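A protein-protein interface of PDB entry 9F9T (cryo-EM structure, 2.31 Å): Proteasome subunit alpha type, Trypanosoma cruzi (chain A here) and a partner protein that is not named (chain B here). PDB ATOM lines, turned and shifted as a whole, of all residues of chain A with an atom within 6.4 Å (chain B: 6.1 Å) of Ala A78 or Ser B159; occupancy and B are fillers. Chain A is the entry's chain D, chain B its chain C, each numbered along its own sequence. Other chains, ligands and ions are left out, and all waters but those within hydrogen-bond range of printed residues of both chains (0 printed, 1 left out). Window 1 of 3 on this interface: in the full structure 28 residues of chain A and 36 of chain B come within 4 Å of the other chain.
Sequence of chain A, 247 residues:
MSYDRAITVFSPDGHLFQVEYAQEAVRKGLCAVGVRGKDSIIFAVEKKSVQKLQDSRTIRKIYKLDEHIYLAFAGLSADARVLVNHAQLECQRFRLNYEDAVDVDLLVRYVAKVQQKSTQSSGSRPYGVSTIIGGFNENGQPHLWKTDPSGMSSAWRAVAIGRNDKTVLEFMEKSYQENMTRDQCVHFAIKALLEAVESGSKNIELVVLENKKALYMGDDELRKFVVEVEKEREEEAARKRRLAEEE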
ATOM      1  N   LYS A  61     -22.361 -29.100 -32.071  1.00  0.00           N
ATOM      2  CA  LYS A  61     -22.143 -29.930 -30.888  1.00  0.00           C
ATOM      3  C   LYS A  61     -20.882 -30.806 -31.029  1.00  0.00           C
ATOM      4  O   LYS A  61     -20.640 -31.745 -30.262  1.00  0.00           O
ATOM      5  CB  LYS A  61     -23.426 -30.738 -30.693  1.00  0.00           C
ATOM      6  CG  LYS A  61     -24.631 -29.872 -30.345  1.00  0.00           C
ATOM      7  CD  LYS A  61     -24.380 -28.975 -29.115  1.00  0.00           C
ATOM      8  CE  LYS A  61     -25.640 -28.572 -28.374  1.00  0.00           C
ATOM      9  NZ  LYS A  61     -25.448 -28.582 -26.903  1.00  0.00           N
ATOM     10  N   PHE A  73     -19.164 -34.922 -27.628  1.00  0.00           N
ATOM     11  CA  PHE A  73     -19.415 -35.350 -26.264  1.00  0.00           C
ATOM     12  C   PHE A  73     -20.824 -35.897 -26.171  1.00  0.00           C
ATOM     13  O   PHE A  73     -21.595 -35.813 -27.114  1.00  0.00           O
ATOM     14  CB  PHE A  73     -19.300 -34.192 -25.272  1.00  0.00           C
ATOM     15  CG  PHE A  73     -20.390 -33.178 -25.439  1.00  0.00           C
ATOM     16  CD1 PHE A  73     -20.268 -32.157 -26.374  1.00  0.00           C
ATOM     17  CD2 PHE A  73     -21.610 -33.351 -24.792  1.00  0.00           C
ATOM     18  CE1 PHE A  73     -21.313 -31.267 -26.575  1.00  0.00           C
ATOM     19  CE2 PHE A  73     -22.664 -32.477 -25.009  1.00  0.00           C
ATOM     20  CZ  PHE A  73     -22.509 -31.432 -25.893  1.00  0.00           C
ATOM     21  N   GLY A  75     -23.742 -35.962 -22.623  1.00  0.00           N
ATOM     22  CA  GLY A  75     -23.934 -35.573 -21.230  1.00  0.00           C
ATOM     23  C   GLY A  75     -24.373 -34.118 -21.110  1.00  0.00           C
ATOM     24  O   GLY A  75     -24.864 -33.523 -22.063  1.00  0.00           O
ATOM     25  N   LEU A  76     -24.127 -33.525 -19.954  1.00  0.00           N
ATOM     26  CA  LEU A  76     -24.471 -32.129 -19.707  1.00  0.00           C
ATOM     27  C   LEU A  76     -23.725 -31.194 -20.660  1.00  0.00           C
ATOM     28  O   LEU A  76     -22.502 -31.048 -20.599  1.00  0.00           O
ATOM     29  CB  LEU A  76     -24.128 -31.825 -18.257  1.00  0.00           C
ATOM     30  CG  LEU A  76     -24.884 -32.671 -17.234  1.00  0.00           C
ATOM     31  CD1 LEU A  76     -24.589 -32.186 -15.796  1.00  0.00           C
ATOM     32  CD2 LEU A  76     -26.361 -32.616 -17.528  1.00  0.00           C
ATOM     33  N   SER A  77     -24.480 -30.562 -21.561  1.00  0.00           N
ATOM     34  CA  SER A  77     -23.857 -29.797 -22.632  1.00  0.00           C
ATOM     35  C   SER A  77     -23.097 -28.584 -22.086  1.00  0.00           C
ATOM     36  O   SER A  77     -22.057 -28.222 -22.598  1.00  0.00           O
ATOM     37  CB  SER A  77     -24.883 -29.430 -23.694  1.00  0.00           C
ATOM     38  OG  SER A  77     -25.765 -28.427 -23.230  1.00  0.00           O
ATOM     39  N   ALA A  78     -23.567 -28.007 -20.994  1.00  0.00           N
ATOM     40  CA  ALA A  78     -22.910 -26.847 -20.417  1.00  0.00           C
ATOM     41  C   ALA A  78     -21.582 -27.209 -19.746  1.00  0.00           C
ATOM     42  O   ALA A  78     -20.603 -26.475 -19.859  1.00  0.00           O
ATOM     43  CB  ALA A  78     -23.852 -26.193 -19.430  1.00  0.00           C
ATOM     44  N   ASP A  79     -21.554 -28.327 -19.027  1.00  0.00           N
ATOM     45  CA  ASP A  79     -20.310 -28.818 -18.467  1.00  0.00           C
ATOM     46  C   ASP A  79     -19.289 -29.038 -19.557  1.00  0.00           C
ATOM     47  O   ASP A  79     -18.119 -28.864 -19.286  1.00  0.00           O
ATOM     48  CB  ASP A  79     -20.481 -30.111 -17.654  1.00  0.00           C
ATOM     49  CG  ASP A  79     -21.116 -29.911 -16.280  1.00  0.00           C
ATOM     50  OD1 ASP A  79     -21.458 -28.755 -15.953  1.00  0.00           O
ATOM     51  OD2 ASP A  79     -21.294 -30.930 -15.550  1.00  0.00           O
ATOM     52  N   ALA A  80     -19.734 -29.445 -20.744  1.00  0.00           N
ATOM     53  CA  ALA A  80     -18.844 -29.856 -21.802  1.00  0.00           C
ATOM     54  C   ALA A  80     -18.171 -28.669 -22.476  1.00  0.00           C
ATOM     55  O   ALA A  80     -17.022 -28.752 -22.953  1.00  0.00           O
ATOM     56  CB  ALA A  80     -19.629 -30.637 -22.831  1.00  0.00           C
ATOM     57  N   ARG A  81     -18.962 -27.612 -22.614  1.00  0.00           N
ATOM     58  CA  ARG A  81     -18.514 -26.318 -23.106  1.00  0.00           C
ATOM     59  C   ARG A  81     -17.388 -25.798 -22.200  1.00  0.00           C
ATOM     60  O   ARG A  81     -16.350 -25.366 -22.655  1.00  0.00           O
ATOM     61  CB  ARG A  81     -19.758 -25.440 -23.193  1.00  0.00           C
ATOM     62  CG  ARG A  81     -19.647 -24.371 -24.255  1.00  0.00           C
ATOM     63  CD  ARG A  81     -20.890 -23.517 -24.311  1.00  0.00           C
ATOM     64  NE  ARG A  81     -21.060 -22.796 -23.062  1.00  0.00           N
ATOM     65  CZ  ARG A  81     -22.105 -22.976 -22.270  1.00  0.00           C
ATOM     66  NH1 ARG A  81     -22.106 -22.449 -21.056  1.00  0.00           N
ATOM     67  NH2 ARG A  81     -23.104 -23.735 -22.697  1.00  0.00           N
ATOM     68  N   VAL A  82     -17.501 -25.990 -20.889  1.00  0.00           N
ATOM     69  CA  VAL A  82     -16.419 -25.605 -19.993  1.00  0.00           C
ATOM     70  C   VAL A  82     -15.199 -26.451 -20.307  1.00  0.00           C
ATOM     71  O   VAL A  82     -14.095 -25.949 -20.545  1.00  0.00           O
ATOM     72  CB  VAL A  82     -16.862 -25.783 -18.537  1.00  0.00           C
ATOM     73  CG1 VAL A  82     -15.744 -25.564 -17.538  1.00  0.00           C
ATOM     74  CG2 VAL A  82     -18.019 -24.869 -18.245  1.00  0.00           C
ATOM     75  N   LEU A  83     -15.413 -27.761 -20.360  1.00  0.00           N
ATOM     76  CA  LEU A  83     -14.326 -28.661 -20.671  1.00  0.00           C
ATOM     77  C   LEU A  83     -13.653 -28.283 -21.978  1.00  0.00           C
ATOM     78  O   LEU A  83     -12.436 -28.176 -21.957  1.00  0.00           O
ATOM     79  CB  LEU A  83     -14.890 -30.062 -20.696  1.00  0.00           C
ATOM     80  CG  LEU A  83     -13.970 -31.177 -20.256  1.00  0.00           C
ATOM     81  CD1 LEU A  83     -13.413 -30.953 -18.854  1.00  0.00           C
ATOM     82  CD2 LEU A  83     -14.743 -32.485 -20.308  1.00  0.00           C
ATOM     83  N   VAL A 129     -19.927 -35.518 -18.210  1.00  0.00           N
ATOM     84  CA  VAL A 129     -19.614 -35.482 -19.620  1.00  0.00           C
ATOM     85  C   VAL A 129     -18.727 -36.667 -19.963  1.00  0.00           C
ATOM     86  O   VAL A 129     -17.820 -36.982 -19.193  1.00  0.00           O
ATOM     87  CB  VAL A 129     -18.823 -34.193 -19.924  1.00  0.00           C
ATOM     88  CG1 VAL A 129     -18.361 -34.202 -21.364  1.00  0.00           C
ATOM     89  CG2 VAL A 129     -19.617 -32.927 -19.642  1.00  0.00           C
ATOM     90  N   VAL B  21     -31.196 -27.049 -10.411  1.00  0.00           N
ATOM     91  CA  VAL B  21     -31.285 -26.585 -11.805  1.00  0.00           C
ATOM     92  C   VAL B  21     -32.693 -26.781 -12.358  1.00  0.00           C
ATOM     93  O   VAL B  21     -33.207 -25.907 -13.055  1.00  0.00           O
ATOM     94  CB  VAL B  21     -30.197 -27.198 -12.726  1.00  0.00           C
ATOM     95  CG1 VAL B  21     -30.376 -26.837 -14.199  1.00  0.00           C
ATOM     96  CG2 VAL B  21     -28.790 -26.780 -12.280  1.00  0.00           C
ATOM     97  N   CYS B 121     -23.848 -17.664 -20.151  1.00  0.00           N
ATOM     98  CA  CYS B 121     -24.195 -19.028 -19.814  1.00  0.00           C
ATOM     99  C   CYS B 121     -23.110 -19.721 -19.016  1.00  0.00           C
ATOM    100  O   CYS B 121     -23.459 -20.533 -18.161  1.00  0.00           O
ATOM    101  CB  CYS B 121     -24.437 -19.814 -21.078  1.00  0.00           C
ATOM    102  SG  CYS B 121     -25.989 -19.287 -21.831  1.00  0.00           S
ATOM    103  N   ASP B 122     -21.837 -19.384 -19.279  1.00  0.00           N
ATOM    104  CA  ASP B 122     -20.727 -19.831 -18.452  1.00  0.00           C
ATOM    105  C   ASP B 122     -20.834 -19.319 -17.025  1.00  0.00           C
ATOM    106  O   ASP B 122     -20.561 -20.052 -16.082  1.00  0.00           O
ATOM    107  CB  ASP B 122     -19.368 -19.346 -18.961  1.00  0.00           C
ATOM    108  CG  ASP B 122     -18.864 -19.986 -20.255  1.00  0.00           C
ATOM    109  OD1 ASP B 122     -19.537 -20.960 -20.784  1.00  0.00           O
ATOM    110  OD2 ASP B 122     -17.792 -19.498 -20.746  1.00  0.00           O
ATOM    111  N   LYS B 124     -23.547 -18.840 -15.521  1.00  0.00           N
ATOM    112  CA  LYS B 124     -24.634 -19.556 -14.879  1.00  0.00           C
ATOM    113  C   LYS B 124     -24.165 -20.950 -14.437  1.00  0.00           C
ATOM    114  O   LYS B 124     -24.488 -21.393 -13.330  1.00  0.00           O
ATOM    115  CB  LYS B 124     -25.819 -19.718 -15.835  1.00  0.00           C
ATOM    116  CG  LYS B 124     -26.509 -18.427 -16.235  1.00  0.00           C
ATOM    117  CD  LYS B 124     -27.962 -18.612 -16.589  1.00  0.00           C
ATOM    118  CE  LYS B 124     -28.399 -17.858 -17.822  1.00  0.00           C
ATOM    119  NZ  LYS B 124     -29.826 -18.164 -18.078  1.00  0.00           N
ATOM    120  N   GLN B 125     -23.430 -21.619 -15.338  1.00  0.00           N
ATOM    121  CA  GLN B 125     -22.929 -22.968 -15.158  1.00  0.00           C
ATOM    122  C   GLN B 125     -22.027 -22.960 -13.937  1.00  0.00           C
ATOM    123  O   GLN B 125     -22.043 -23.915 -13.170  1.00  0.00           O
ATOM    124  CB  GLN B 125     -22.248 -23.461 -16.436  1.00  0.00           C
ATOM    125  CG  GLN B 125     -21.711 -24.898 -16.398  1.00  0.00           C
ATOM    126  CD  GLN B 125     -20.374 -25.100 -15.712  1.00  0.00           C
ATOM    127  OE1 GLN B 125     -19.533 -24.208 -15.590  1.00  0.00           O
ATOM    128  NE2 GLN B 125     -20.153 -26.327 -15.277  1.00  0.00           N
ATOM    129  N   THR B 128     -23.632 -23.917 -10.894  1.00  0.00           N
ATOM    130  CA  THR B 128     -24.131 -25.285 -10.840  1.00  0.00           C
ATOM    131  C   THR B 128     -23.047 -26.272 -10.375  1.00  0.00           C
ATOM    132  O   THR B 128     -23.365 -27.330  -9.827  1.00  0.00           O
ATOM    133  CB  THR B 128     -24.761 -25.726 -12.178  1.00  0.00           C
ATOM    134  OG1 THR B 128     -23.743 -26.045 -13.143  1.00  0.00           O
ATOM    135  CG2 THR B 128     -25.719 -24.685 -12.740  1.00  0.00           C
ATOM    136  N   ASP B 157     -30.951 -20.958 -20.751  1.00  0.00           N
ATOM    137  CA  ASP B 157     -31.808 -21.658 -19.818  1.00  0.00           C
ATOM    138  C   ASP B 157     -31.045 -21.804 -18.500  1.00  0.00           C
ATOM    139  O   ASP B 157     -29.853 -21.514 -18.458  1.00  0.00           O
ATOM    140  CB  ASP B 157     -32.295 -22.945 -20.483  1.00  0.00           C
ATOM    141  CG  ASP B 157     -31.273 -24.064 -20.537  1.00  0.00           C
ATOM    142  OD1 ASP B 157     -30.344 -24.074 -19.714  1.00  0.00           O
ATOM    143  OD2 ASP B 157     -31.454 -24.962 -21.415  1.00  0.00           O
ATOM    144  N   THR B 158     -31.698 -22.245 -17.429  1.00  0.00           N
ATOM    145  CA  THR B 158     -31.023 -22.169 -16.150  1.00  0.00           C
ATOM    146  C   THR B 158     -29.767 -23.035 -16.049  1.00  0.00           C
ATOM    147  O   THR B 158     -29.022 -22.874 -15.082  1.00  0.00           O
ATOM    148  CB  THR B 158     -31.945 -22.604 -15.019  1.00  0.00           C
ATOM    149  OG1 THR B 158     -32.292 -23.978 -15.195  1.00  0.00           O
ATOM    150  CG2 THR B 158     -33.175 -21.744 -14.983  1.00  0.00           C
ATOM    151  N   SER B 159     -29.562 -23.981 -16.991  1.00  0.00           N
ATOM    152  CA  SER B 159     -28.484 -24.954 -16.912  1.00  0.00           C
ATOM    153  C   SER B 159     -27.188 -24.325 -17.370  1.00  0.00           C
ATOM    154  O   SER B 159     -26.097 -24.853 -17.151  1.00  0.00           O
ATOM    155  CB  SER B 159     -28.772 -26.199 -17.743  1.00  0.00           C
ATOM    156  OG  SER B 159     -29.302 -25.897 -19.034  1.00  0.00           O
ATOM    157  N   GLY B 160     -27.332 -23.203 -18.058  1.00  0.00           N
ATOM    158  CA  GLY B 160     -26.206 -22.598 -18.714  1.00  0.00           C
ATOM    159  C   GLY B 160     -26.113 -23.097 -20.137  1.00  0.00           C
ATOM    160  O   GLY B 160     -25.027 -23.096 -20.699  1.00  0.00           O
ATOM    161  N   ASN B 161     -27.242 -23.540 -20.674  1.00  0.00           N
ATOM    162  CA  ASN B 161     -27.377 -23.946 -22.058  1.00  0.00           C
ATOM    163  C   ASN B 161     -28.005 -22.856 -22.907  1.00  0.00           C
ATOM    164  O   ASN B 161     -28.845 -22.129 -22.420  1.00  0.00           O
ATOM    165  CB  ASN B 161     -28.403 -25.063 -22.231  1.00  0.00           C
ATOM    166  CG  ASN B 161     -27.761 -26.330 -22.704  1.00  0.00           C
ATOM    167  OD1 ASN B 161     -27.581 -26.510 -23.912  1.00  0.00           O
ATOM    168  ND2 ASN B 161     -27.411 -27.183 -21.752  1.00  0.00           N
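Printed residues of chain B within 4 Å of Ala A78: Gln B125, Ser B159 and Gly B160.
Ser B159 touches just one residue of chain A: Ala A78.
Of the printed residues of chain B, Arg A81 touches Cys B121 (3.5 Å), Asp B122 (3.0 Å) and Gly B160 (2.8 Å).
Of the printed residues of chain A, Cys B121 touches Arg A81.
Of the printed residues of chain A, Asn B161 touches Ser A77.
Of the printed residues of chain B, Asp A79 touches Gln B125.
CG of Gln B125 touches CB of Ala A78, at 3.9 Å.
Ala A78 touches Ser B159.
O of Gly B160 touches CB of Ala A78 (3.5 Å).
Arg A81 touches Cys B121.
Val A82 touches Gln B125 (CG2 to OE1, 3.1 Å).
The guanidinium group (NH1) of Arg A81 lies within salt-bridge range of the side-chain carboxylate (OD1) of Asp B122 (3.0 Å).
NE2 of Gln B125 sits at hydrogen-bond distance from OD1 of Asp A79, at 2.8 Å.
O of Gly B160 sits at hydrogen-bond distance from NH2 of Arg A81.
The side-chain amide nitrogen (ND2) of Asn B161 is in hydrogen-bond range of the side-chain hydroxyl (OG) of Ser A77 (2.5 Å).
Of the 11 printed residues of chain B, 6 touch a printed residue of chain A.
Printed residues of chain B that touch a printed residue of chain A: Cys B121, Asp B122, Gln B125, Ser B159, Gly B160 and Asn B161.
Of the 12 printed residues of chain A, 5 touch a printed residue of chain B.
Printed residues of chain A that touch a printed residue of chain B: Ser A77, Ala A78, Asp A79, Arg A81 and Val A82.
Hydrophobic or aromatic side chains of chain A that line the printed part of chain B: Ala A78 and Val A82.
Along chain A the printed residues that touch a printed residue of chain B span positions 77 to 82.
Among the printed residues, 9 pairs touch across the chains.
Among the printed residues, Asp or Glu carboxylates within 4 Å of a Lys or Arg side-chain nitrogen of the other chain: Arg A81 with Asp B122 (3.0 Å).
The backbone carbonyl oxygen of Gln B125 sits at hydrogen-bond distance from the side-chain hydroxyl of Thr B128 (2.7 Å).
N of Ser B159 lies within hydrogen-bond range of OD1 of Asp B157, 2.8 Å away.
The backbone NH (N) of Asn B161 lies within hydrogen-bond range of the side-chain carboxylate (OD1) of Asp B157 (3.3 Å).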
